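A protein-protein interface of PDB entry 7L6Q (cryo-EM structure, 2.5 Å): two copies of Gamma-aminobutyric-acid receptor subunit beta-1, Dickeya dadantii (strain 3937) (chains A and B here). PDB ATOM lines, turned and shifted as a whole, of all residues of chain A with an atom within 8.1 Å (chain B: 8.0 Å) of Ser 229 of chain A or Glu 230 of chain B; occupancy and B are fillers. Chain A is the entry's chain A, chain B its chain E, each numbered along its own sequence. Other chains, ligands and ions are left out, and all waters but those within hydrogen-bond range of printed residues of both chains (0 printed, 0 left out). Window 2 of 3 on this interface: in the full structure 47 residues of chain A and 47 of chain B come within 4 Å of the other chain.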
ATOM      1  N   LEU A 225      27.304   0.089 -18.882  1.00  0.00           N
ATOM      2  CA  LEU A 225      28.151  -0.619 -19.822  1.00  0.00           C
ATOM      3  C   LEU A 225      28.479   0.291 -20.999  1.00  0.00           C
ATOM      4  O   LEU A 225      27.768   1.256 -21.283  1.00  0.00           O
ATOM      5  CB  LEU A 225      27.465  -1.892 -20.298  1.00  0.00           C
ATOM      6  CG  LEU A 225      27.162  -2.899 -19.199  1.00  0.00           C
ATOM      7  CD1 LEU A 225      26.250  -3.973 -19.708  1.00  0.00           C
ATOM      8  CD2 LEU A 225      28.441  -3.506 -18.713  1.00  0.00           C
ATOM      9  N   GLU A 226      29.572  -0.012 -21.684  1.00  0.00           N
ATOM     10  CA  GLU A 226      30.142   0.909 -22.656  1.00  0.00           C
ATOM     11  C   GLU A 226      30.175   0.326 -24.061  1.00  0.00           C
ATOM     12  O   GLU A 226      31.112   0.560 -24.824  1.00  0.00           O
ATOM     13  CB  GLU A 226      31.539   1.334 -22.225  1.00  0.00           C
ATOM     14  CG  GLU A 226      31.553   2.138 -20.949  1.00  0.00           C
ATOM     15  CD  GLU A 226      32.952   2.405 -20.446  1.00  0.00           C
ATOM     16  OE1 GLU A 226      33.878   1.669 -20.843  1.00  0.00           O
ATOM     17  OE2 GLU A 226      33.126   3.354 -19.652  1.00  0.00           O
ATOM     18  N   SER A 227      29.150  -0.433 -24.432  1.00  0.00           N
ATOM     19  CA  SER A 227      29.063  -0.982 -25.776  1.00  0.00           C
ATOM     20  C   SER A 227      27.610  -1.291 -26.080  1.00  0.00           C
ATOM     21  O   SER A 227      26.868  -1.715 -25.195  1.00  0.00           O
ATOM     22  CB  SER A 227      29.907  -2.249 -25.924  1.00  0.00           C
ATOM     23  OG  SER A 227      31.279  -1.981 -25.700  1.00  0.00           O
ATOM     24  N   PHE A 228      27.208  -1.077 -27.331  1.00  0.00           N
ATOM     25  CA  PHE A 228      25.844  -1.413 -27.713  1.00  0.00           C
ATOM     26  C   PHE A 228      25.590  -2.904 -27.583  1.00  0.00           C
ATOM     27  O   PHE A 228      24.518  -3.320 -27.132  1.00  0.00           O
ATOM     28  CB  PHE A 228      25.555  -0.954 -29.136  1.00  0.00           C
ATOM     29  CG  PHE A 228      24.323  -1.568 -29.719  1.00  0.00           C
ATOM     30  CD1 PHE A 228      23.087  -1.299 -29.186  1.00  0.00           C
ATOM     31  CD2 PHE A 228      24.404  -2.419 -30.791  1.00  0.00           C
ATOM     32  CE1 PHE A 228      21.965  -1.865 -29.712  1.00  0.00           C
ATOM     33  CE2 PHE A 228      23.278  -2.982 -31.316  1.00  0.00           C
ATOM     34  CZ  PHE A 228      22.061  -2.704 -30.776  1.00  0.00           C
ATOM     35  N   SER A 229      26.558  -3.728 -27.979  1.00  0.00           N
ATOM     36  CA  SER A 229      26.366  -5.168 -27.897  1.00  0.00           C
ATOM     37  C   SER A 229      26.241  -5.638 -26.458  1.00  0.00           C
ATOM     38  O   SER A 229      25.467  -6.554 -26.177  1.00  0.00           O
ATOM     39  CB  SER A 229      27.511  -5.893 -28.592  1.00  0.00           C
ATOM     40  OG  SER A 229      28.749  -5.557 -28.001  1.00  0.00           O
ATOM     41  N   GLU A 230      26.986  -5.033 -25.534  1.00  0.00           N
ATOM     42  CA  GLU A 230      26.913  -5.456 -24.142  1.00  0.00           C
ATOM     43  C   GLU A 230      25.610  -5.025 -23.487  1.00  0.00           C
ATOM     44  O   GLU A 230      25.040  -5.775 -22.691  1.00  0.00           O
ATOM     45  CB  GLU A 230      28.095  -4.898 -23.362  1.00  0.00           C
ATOM     46  CG  GLU A 230      29.426  -5.374 -23.861  1.00  0.00           C
ATOM     47  CD  GLU A 230      30.570  -4.600 -23.259  1.00  0.00           C
ATOM     48  OE1 GLU A 230      30.311  -3.720 -22.416  1.00  0.00           O
ATOM     49  OE2 GLU A 230      31.731  -4.868 -23.627  1.00  0.00           O
ATOM     50  N   ARG A 231      25.128  -3.824 -23.796  1.00  0.00           N
ATOM     51  CA  ARG A 231      23.899  -3.349 -23.176  1.00  0.00           C
ATOM     52  C   ARG A 231      22.707  -4.195 -23.591  1.00  0.00           C
ATOM     53  O   ARG A 231      21.828  -4.480 -22.773  1.00  0.00           O
ATOM     54  CB  ARG A 231      23.666  -1.885 -23.524  1.00  0.00           C
ATOM     55  CG  ARG A 231      24.677  -0.960 -22.908  1.00  0.00           C
ATOM     56  CD  ARG A 231      24.214   0.465 -22.962  1.00  0.00           C
ATOM     57  NE  ARG A 231      24.410   1.052 -24.272  1.00  0.00           N
ATOM     58  CZ  ARG A 231      25.386   1.899 -24.561  1.00  0.00           C
ATOM     59  NH1 ARG A 231      26.246   2.254 -23.626  1.00  0.00           N
ATOM     60  NH2 ARG A 231      25.497   2.393 -25.780  1.00  0.00           N
ATOM     61  N   LEU A 232      22.656  -4.604 -24.855  1.00  0.00           N
ATOM     62  CA  LEU A 232      21.515  -5.377 -25.323  1.00  0.00           C
ATOM     63  C   LEU A 232      21.530  -6.792 -24.766  1.00  0.00           C
ATOM     64  O   LEU A 232      20.485  -7.318 -24.373  1.00  0.00           O
ATOM     65  CB  LEU A 232      21.496  -5.404 -26.846  1.00  0.00           C
ATOM     66  CG  LEU A 232      20.193  -4.963 -27.491  1.00  0.00           C
ATOM     67  CD1 LEU A 232      20.273  -5.127 -28.977  1.00  0.00           C
ATOM     68  CD2 LEU A 232      19.060  -5.773 -26.944  1.00  0.00           C
ATOM     69  N   GLN A 233      22.701  -7.427 -24.723  1.00  0.00           N
ATOM     70  CA  GLN A 233      22.757  -8.823 -24.303  1.00  0.00           C
ATOM     71  C   GLN A 233      22.453  -8.977 -22.820  1.00  0.00           C
ATOM     72  O   GLN A 233      21.795  -9.940 -22.418  1.00  0.00           O
ATOM     73  CB  GLN A 233      24.116  -9.421 -24.637  1.00  0.00           C
ATOM     74  CG  GLN A 233      24.399  -9.473 -26.112  1.00  0.00           C
ATOM     75  CD  GLN A 233      25.650 -10.243 -26.428  1.00  0.00           C
ATOM     76  OE1 GLN A 233      25.975 -11.218 -25.757  1.00  0.00           O
ATOM     77  NE2 GLN A 233      26.367  -9.810 -27.452  1.00  0.00           N
ATOM     78  N   THR A 234      22.922  -8.050 -21.989  1.00  0.00           N
ATOM     79  CA  THR A 234      22.627  -8.149 -20.568  1.00  0.00           C
ATOM     80  C   THR A 234      21.212  -7.722 -20.231  1.00  0.00           C
ATOM     81  O   THR A 234      20.777  -7.932 -19.096  1.00  0.00           O
ATOM     82  CB  THR A 234      23.607  -7.315 -19.752  1.00  0.00           C
ATOM     83  OG1 THR A 234      23.390  -5.930 -20.023  1.00  0.00           O
ATOM     84  CG2 THR A 234      25.015  -7.672 -20.121  1.00  0.00           C
ATOM     85  N   SER A 235      20.487  -7.123 -21.173  1.00  0.00           N
ATOM     86  CA  SER A 235      19.082  -6.837 -20.932  1.00  0.00           C
ATOM     87  C   SER A 235      18.244  -8.101 -20.975  1.00  0.00           C
ATOM     88  O   SER A 235      17.219  -8.184 -20.292  1.00  0.00           O
ATOM     89  CB  SER A 235      18.564  -5.827 -21.945  1.00  0.00           C
ATOM     90  OG  SER A 235      19.037  -4.533 -21.643  1.00  0.00           O
ATOM     91  N   PHE A 236      18.652  -9.090 -21.767  1.00  0.00           N
ATOM     92  CA  PHE A 236      17.905 -10.337 -21.823  1.00  0.00           C
ATOM     93  C   PHE A 236      18.141 -11.195 -20.593  1.00  0.00           C
ATOM     94  O   PHE A 236      17.243 -11.938 -20.185  1.00  0.00           O
ATOM     95  CB  PHE A 236      18.265 -11.108 -23.085  1.00  0.00           C
ATOM     96  CG  PHE A 236      17.952 -10.370 -24.340  1.00  0.00           C
ATOM     97  CD1 PHE A 236      16.667  -9.989 -24.619  1.00  0.00           C
ATOM     98  CD2 PHE A 236      18.941 -10.060 -25.239  1.00  0.00           C
ATOM     99  CE1 PHE A 236      16.378  -9.309 -25.764  1.00  0.00           C
ATOM    100  CE2 PHE A 236      18.653  -9.381 -26.386  1.00  0.00           C
ATOM    101  CZ  PHE A 236      17.371  -9.007 -26.648  1.00  0.00           C
ATOM    102  N   ILE A 280      18.140   1.675 -25.647  1.00  0.00           N
ATOM    103  CA  ILE A 280      19.459   1.210 -26.063  1.00  0.00           C
ATOM    104  C   ILE A 280      19.530   1.108 -27.578  1.00  0.00           C
ATOM    105  O   ILE A 280      20.506   1.538 -28.200  1.00  0.00           O
ATOM    106  CB  ILE A 280      19.788  -0.135 -25.399  1.00  0.00           C
ATOM    107  CG1 ILE A 280      19.946   0.042 -23.901  1.00  0.00           C
ATOM    108  CG2 ILE A 280      21.049  -0.701 -25.973  1.00  0.00           C
ATOM    109  CD1 ILE A 280      20.060  -1.251 -23.169  1.00  0.00           C
ATOM    110  N   HIS A 284      21.502   3.810 -30.394  1.00  0.00           N
ATOM    111  CA  HIS A 284      22.543   3.283 -31.261  1.00  0.00           C
ATOM    112  C   HIS A 284      22.256   3.513 -32.733  1.00  0.00           C
ATOM    113  O   HIS A 284      23.193   3.676 -33.518  1.00  0.00           O
ATOM    114  CB  HIS A 284      22.718   1.786 -30.999  1.00  0.00           C
ATOM    115  CG  HIS A 284      23.684   1.111 -31.920  1.00  0.00           C
ATOM    116  ND1 HIS A 284      25.013   1.462 -31.993  1.00  0.00           N
ATOM    117  CD2 HIS A 284      23.515   0.095 -32.796  1.00  0.00           C
ATOM    118  CE1 HIS A 284      25.620   0.696 -32.880  1.00  0.00           C
ATOM    119  NE2 HIS A 284      24.734  -0.142 -33.382  1.00  0.00           N
ATOM    120  N   VAL A 291      26.506   5.517 -32.288  1.00  0.00           N
ATOM    121  CA  VAL A 291      27.378   4.797 -31.362  1.00  0.00           C
ATOM    122  C   VAL A 291      28.574   5.630 -30.935  1.00  0.00           C
ATOM    123  O   VAL A 291      29.327   5.213 -30.045  1.00  0.00           O
ATOM    124  CB  VAL A 291      27.847   3.472 -31.995  1.00  0.00           C
ATOM    125  CG1 VAL A 291      29.015   3.713 -32.944  1.00  0.00           C
ATOM    126  CG2 VAL A 291      28.204   2.449 -30.921  1.00  0.00           C
ATOM    127  N   VAL B 222      16.667  -9.109 -31.609  1.00  0.00           N
ATOM    128  CA  VAL B 222      17.866  -9.851 -31.956  1.00  0.00           C
ATOM    129  C   VAL B 222      18.364  -9.496 -33.346  1.00  0.00           C
ATOM    130  O   VAL B 222      19.518  -9.780 -33.676  1.00  0.00           O
ATOM    131  CB  VAL B 222      17.598 -11.359 -31.834  1.00  0.00           C
ATOM    132  CG1 VAL B 222      16.854 -11.859 -33.043  1.00  0.00           C
ATOM    133  CG2 VAL B 222      18.886 -12.108 -31.653  1.00  0.00           C
ATOM    134  N   TRP B 224      18.868  -6.521 -34.391  1.00  0.00           N
ATOM    135  CA  TRP B 224      19.575  -5.256 -34.329  1.00  0.00           C
ATOM    136  C   TRP B 224      21.013  -5.405 -33.866  1.00  0.00           C
ATOM    137  O   TRP B 224      21.779  -4.445 -33.969  1.00  0.00           O
ATOM    138  CB  TRP B 224      18.827  -4.284 -33.415  1.00  0.00           C
ATOM    139  CG  TRP B 224      17.465  -3.947 -33.923  1.00  0.00           C
ATOM    140  CD1 TRP B 224      16.324  -4.665 -33.748  1.00  0.00           C
ATOM    141  CD2 TRP B 224      17.100  -2.807 -34.696  1.00  0.00           C
ATOM    142  NE1 TRP B 224      15.272  -4.045 -34.361  1.00  0.00           N
ATOM    143  CE2 TRP B 224      15.725  -2.898 -34.952  1.00  0.00           C
ATOM    144  CE3 TRP B 224      17.805  -1.716 -35.197  1.00  0.00           C
ATOM    145  CZ2 TRP B 224      15.045  -1.946 -35.682  1.00  0.00           C
ATOM    146  CZ3 TRP B 224      17.128  -0.774 -35.921  1.00  0.00           C
ATOM    147  CH2 TRP B 224      15.763  -0.892 -36.159  1.00  0.00           C
ATOM    148  N   LEU B 225      21.397  -6.573 -33.366  1.00  0.00           N
ATOM    149  CA  LEU B 225      22.797  -6.847 -33.105  1.00  0.00           C
ATOM    150  C   LEU B 225      23.555  -6.929 -34.424  1.00  0.00           C
ATOM    151  O   LEU B 225      22.977  -7.176 -35.482  1.00  0.00           O
ATOM    152  CB  LEU B 225      22.946  -8.138 -32.314  1.00  0.00           C
ATOM    153  CG  LEU B 225      22.280  -8.126 -30.945  1.00  0.00           C
ATOM    154  CD1 LEU B 225      22.237  -9.509 -30.371  1.00  0.00           C
ATOM    155  CD2 LEU B 225      23.041  -7.220 -30.030  1.00  0.00           C
ATOM    156  N   GLU B 226      24.861  -6.711 -34.359  1.00  0.00           N
ATOM    157  CA  GLU B 226      25.657  -6.502 -35.561  1.00  0.00           C
ATOM    158  C   GLU B 226      26.743  -7.556 -35.730  1.00  0.00           C
ATOM    159  O   GLU B 226      27.845  -7.263 -36.189  1.00  0.00           O
ATOM    160  CB  GLU B 226      26.270  -5.107 -35.551  1.00  0.00           C
ATOM    161  CG  GLU B 226      25.244  -4.004 -35.630  1.00  0.00           C
ATOM    162  CD  GLU B 226      25.851  -2.633 -35.449  1.00  0.00           C
ATOM    163  OE1 GLU B 226      26.965  -2.544 -34.891  1.00  0.00           O
ATOM    164  OE2 GLU B 226      25.215  -1.643 -35.868  1.00  0.00           O
ATOM    165  N   SER B 227      26.445  -8.801 -35.375  1.00  0.00           N
ATOM    166  CA  SER B 227      27.395  -9.886 -35.559  1.00  0.00           C
ATOM    167  C   SER B 227      26.631 -11.195 -35.615  1.00  0.00           C
ATOM    168  O   SER B 227      25.637 -11.363 -34.908  1.00  0.00           O
ATOM    169  CB  SER B 227      28.427  -9.932 -34.430  1.00  0.00           C
ATOM    170  OG  SER B 227      29.195  -8.744 -34.391  1.00  0.00           O
ATOM    171  N   PHE B 228      27.096 -12.119 -36.453  1.00  0.00           N
ATOM    172  CA  PHE B 228      26.453 -13.423 -36.511  1.00  0.00           C
ATOM    173  C   PHE B 228      26.576 -14.154 -35.185  1.00  0.00           C
ATOM    174  O   PHE B 228      25.626 -14.801 -34.737  1.00  0.00           O
ATOM    175  CB  PHE B 228      27.045 -14.267 -37.632  1.00  0.00           C
ATOM    176  CG  PHE B 228      26.700 -15.717 -37.530  1.00  0.00           C
ATOM    177  CD1 PHE B 228      25.401 -16.137 -37.654  1.00  0.00           C
ATOM    178  CD2 PHE B 228      27.674 -16.655 -37.301  1.00  0.00           C
ATOM    179  CE1 PHE B 228      25.084 -17.459 -37.553  1.00  0.00           C
ATOM    180  CE2 PHE B 228      27.354 -17.978 -37.202  1.00  0.00           C
ATOM    181  CZ  PHE B 228      26.059 -18.377 -37.328  1.00  0.00           C
ATOM    182  N   SER B 229      27.741 -14.072 -34.547  1.00  0.00           N
ATOM    183  CA  SER B 229      27.927 -14.767 -33.281  1.00  0.00           C
ATOM    184  C   SER B 229      27.030 -14.203 -32.193  1.00  0.00           C
ATOM    185  O   SER B 229      26.533 -14.959 -31.355  1.00  0.00           O
ATOM    186  CB  SER B 229      29.386 -14.699 -32.851  1.00  0.00           C
ATOM    187  OG  SER B 229      29.803 -13.357 -32.708  1.00  0.00           O
ATOM    188  N   GLU B 230      26.809 -12.891 -32.181  1.00  0.00           N
ATOM    189  CA  GLU B 230      25.966 -12.299 -31.150  1.00  0.00           C
ATOM    190  C   GLU B 230      24.496 -12.626 -31.363  1.00  0.00           C
ATOM    191  O   GLU B 230      23.769 -12.864 -30.397  1.00  0.00           O
ATOM    192  CB  GLU B 230      26.162 -10.790 -31.114  1.00  0.00           C
ATOM    193  CG  GLU B 230      27.565 -10.373 -30.783  1.00  0.00           C
ATOM    194  CD  GLU B 230      27.793  -8.902 -31.024  1.00  0.00           C
ATOM    195  OE1 GLU B 230      26.832  -8.210 -31.410  1.00  0.00           O
ATOM    196  OE2 GLU B 230      28.933  -8.436 -30.830  1.00  0.00           O
ATOM    197  N   ARG B 231      24.037 -12.627 -32.613  1.00  0.00           N
ATOM    198  CA  ARG B 231      22.632 -12.905 -32.872  1.00  0.00           C
ATOM    199  C   ARG B 231      22.266 -14.328 -32.483  1.00  0.00           C
ATOM    200  O   ARG B 231      21.182 -14.570 -31.947  1.00  0.00           O
ATOM    201  CB  ARG B 231      22.307 -12.649 -34.338  1.00  0.00           C
ATOM    202  CG  ARG B 231      22.391 -11.199 -34.720  1.00  0.00           C
ATOM    203  CD  ARG B 231      21.722 -10.942 -36.036  1.00  0.00           C
ATOM    204  NE  ARG B 231      22.558 -11.332 -37.157  1.00  0.00           N
ATOM    205  CZ  ARG B 231      23.222 -10.472 -37.913  1.00  0.00           C
ATOM    206  NH1 ARG B 231      23.141  -9.180 -37.664  1.00  0.00           N
ATOM    207  NH2 ARG B 231      23.962 -10.906 -38.917  1.00  0.00           N
ATOM    208  N   LEU B 232      23.153 -15.282 -32.745  1.00  0.00           N
ATOM    209  CA  LEU B 232      22.841 -16.671 -32.440  1.00  0.00           C
ATOM    210  C   LEU B 232      22.861 -16.931 -30.942  1.00  0.00           C
ATOM    211  O   LEU B 232      21.995 -17.641 -30.421  1.00  0.00           O
ATOM    212  CB  LEU B 232      23.819 -17.592 -33.156  1.00  0.00           C
ATOM    213  CG  LEU B 232      23.186 -18.681 -34.007  1.00  0.00           C
ATOM    214  CD1 LEU B 232      24.249 -19.572 -34.574  1.00  0.00           C
ATOM    215  CD2 LEU B 232      22.233 -19.480 -33.176  1.00  0.00           C
ATOM    216  N   GLN B 233      23.838 -16.372 -30.229  1.00  0.00           N
ATOM    217  CA  GLN B 233      23.970 -16.678 -28.810  1.00  0.00           C
ATOM    218  C   GLN B 233      22.835 -16.078 -27.996  1.00  0.00           C
ATOM    219  O   GLN B 233      22.355 -16.702 -27.045  1.00  0.00           O
ATOM    220  CB  GLN B 233      25.317 -16.196 -28.288  1.00  0.00           C
ATOM    221  CG  GLN B 233      26.487 -16.893 -28.923  1.00  0.00           C
ATOM    222  CD  GLN B 233      27.790 -16.548 -28.258  1.00  0.00           C
ATOM    223  OE1 GLN B 233      27.842 -16.342 -27.050  1.00  0.00           O
ATOM    224  NE2 GLN B 233      28.852 -16.475 -29.042  1.00  0.00           N
ATOM    225  N   THR B 234      22.391 -14.872 -28.340  1.00  0.00           N
ATOM    226  CA  THR B 234      21.287 -14.278 -27.603  1.00  0.00           C
ATOM    227  C   THR B 234      19.943 -14.870 -27.980  1.00  0.00           C
ATOM    228  O   THR B 234      18.952 -14.588 -27.302  1.00  0.00           O
ATOM    229  CB  THR B 234      21.243 -12.770 -27.813  1.00  0.00           C
ATOM    230  OG1 THR B 234      20.901 -12.490 -29.172  1.00  0.00           O
ATOM    231  CG2 THR B 234      22.584 -12.171 -27.513  1.00  0.00           C
ATOM    232  N   SER B 235      19.877 -15.669 -29.043  1.00  0.00           N
ATOM    233  CA  SER B 235      18.638 -16.370 -29.344  1.00  0.00           C
ATOM    234  C   SER B 235      18.395 -17.509 -28.369  1.00  0.00           C
ATOM    235  O   SER B 235      17.241 -17.845 -28.090  1.00  0.00           O
ATOM    236  CB  SER B 235      18.659 -16.895 -30.772  1.00  0.00           C
ATOM    237  OG  SER B 235      18.464 -15.843 -31.690  1.00  0.00           O
ATOM    238  N   PHE B 236      19.458 -18.115 -27.846  1.00  0.00           N
ATOM    239  CA  PHE B 236      19.285 -19.190 -26.882  1.00  0.00           C
ATOM    240  C   PHE B 236      18.883 -18.668 -25.514  1.00  0.00           C
ATOM    241  O   PHE B 236      18.170 -19.358 -24.780  1.00  0.00           O
ATOM    242  CB  PHE B 236      20.561 -20.014 -26.780  1.00  0.00           C
ATOM    243  CG  PHE B 236      20.955 -20.657 -28.065  1.00  0.00           C
ATOM    244  CD1 PHE B 236      20.114 -21.542 -28.686  1.00  0.00           C
ATOM    245  CD2 PHE B 236      22.166 -20.376 -28.649  1.00  0.00           C
ATOM    246  CE1 PHE B 236      20.471 -22.128 -29.864  1.00  0.00           C
ATOM    247  CE2 PHE B 236      22.521 -20.964 -29.827  1.00  0.00           C
ATOM    248  CZ  PHE B 236      21.675 -21.839 -30.433  1.00  0.00           C
ATOM    249  N   ILE B 280      18.789 -16.185 -39.117  1.00  0.00           N
ATOM    250  CA  ILE B 280      20.125 -15.722 -38.755  1.00  0.00           C
ATOM    251  C   ILE B 280      21.182 -16.610 -39.392  1.00  0.00           C
ATOM    252  O   ILE B 280      22.172 -16.125 -39.947  1.00  0.00           O
ATOM    253  CB  ILE B 280      20.282 -15.676 -37.229  1.00  0.00           C
ATOM    254  CG1 ILE B 280      19.380 -14.608 -36.638  1.00  0.00           C
ATOM    255  CG2 ILE B 280      21.705 -15.388 -36.864  1.00  0.00           C
ATOM    256  CD1 ILE B 280      19.327 -14.647 -35.150  1.00  0.00           C
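A ring nitrogen (NE2) of His 284 of chain A sits at hydrogen-bond distance from the side-chain carboxylate of Glu 226 of chain B (2.9 Å).
Among the printed residues, merely in contact across the chains: Phe 228 of chain A with Trp 224 of chain B, Gln 233 of chain A with Thr 234 of chain B, Gln 233 of chain A with Glu 230 of chain B, Leu 232 of chain A with Leu 225 of chain B and Ser 229 of chain A with Glu 230 of chain B.
Ser 229 of chain A touches one residue of chain B.
Glu 230 of chain B touches two residues of chain A.
Printed residues of chain A within 4 Å of Leu 225 of chain B: Leu 232 (3.6 Å).
Printed residues of chain B within 4 Å of Gln 233 of chain A: Glu 230 and Thr 234.
Of the printed residues of chain B, Leu 232 of chain A touches Leu 225 (3.6 Å).
Thr 234 of chain A touches none of the printed residues of chain B.
The nearest residue of chain B that does not touch Ser 229 of chain A is Leu 225 of chain B (4.5 Å).
The nearest residue of chain A that does not touch Glu 230 of chain B is Phe 228 of chain A (6.3 Å).
The nearest printed residue of chain B that does not touch Phe 228 of chain A is Leu 225 of chain B (4.3 Å).
Ser 229 of chain A touches Glu 230 of chain B, but with the chains exchanged Glu 230 of chain A does not touch Ser 229 of chain B (11.3 Å).
Leu 232 of chain A touches Leu 225 of chain B, but with the chains exchanged Leu 225 of chain A does not touch Leu 232 of chain B (17.5 Å).
Gln 233 of chain A touches Glu 230 of chain B, but with the chains exchanged Glu 230 of chain A does not touch Gln 233 of chain B (11.3 Å).
Gln 233 of chain A touches Thr 234 of chain B, but with the chains exchanged Thr 234 of chain A does not touch Gln 233 of chain B (10.0 Å).
Of the 6 pairs that touch across the chains among the printed residues, none has its exchanged pair printed and touching as well.
Of the 15 printed residues of chain B, 5 touch a printed residue of chain A.
Hydrophobic or aromatic side chains of chain A within 4 Å of the printed part of chain B: Phe 228, Leu 232 and His 284.
Among the printed residues, no Asp or Glu carboxylate lies within 4 Å of a Lys or Arg side-chain nitrogen of the other chain.
O of Leu 225 of chain B sits at hydrogen-bond distance from NH1 of Arg 231 of chain B (3.0 Å).
The backbone carbonyl oxygen (O) of Glu 230 of chain B is in hydrogen-bond range of the side-chain hydroxyl (OG1) of Thr 234 of chain B.
The backbone carbonyl oxygen of Arg 231 of chain B lies within hydrogen-bond range of the side-chain hydroxyl of Thr 234 of chain B, 3.5 Å away.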
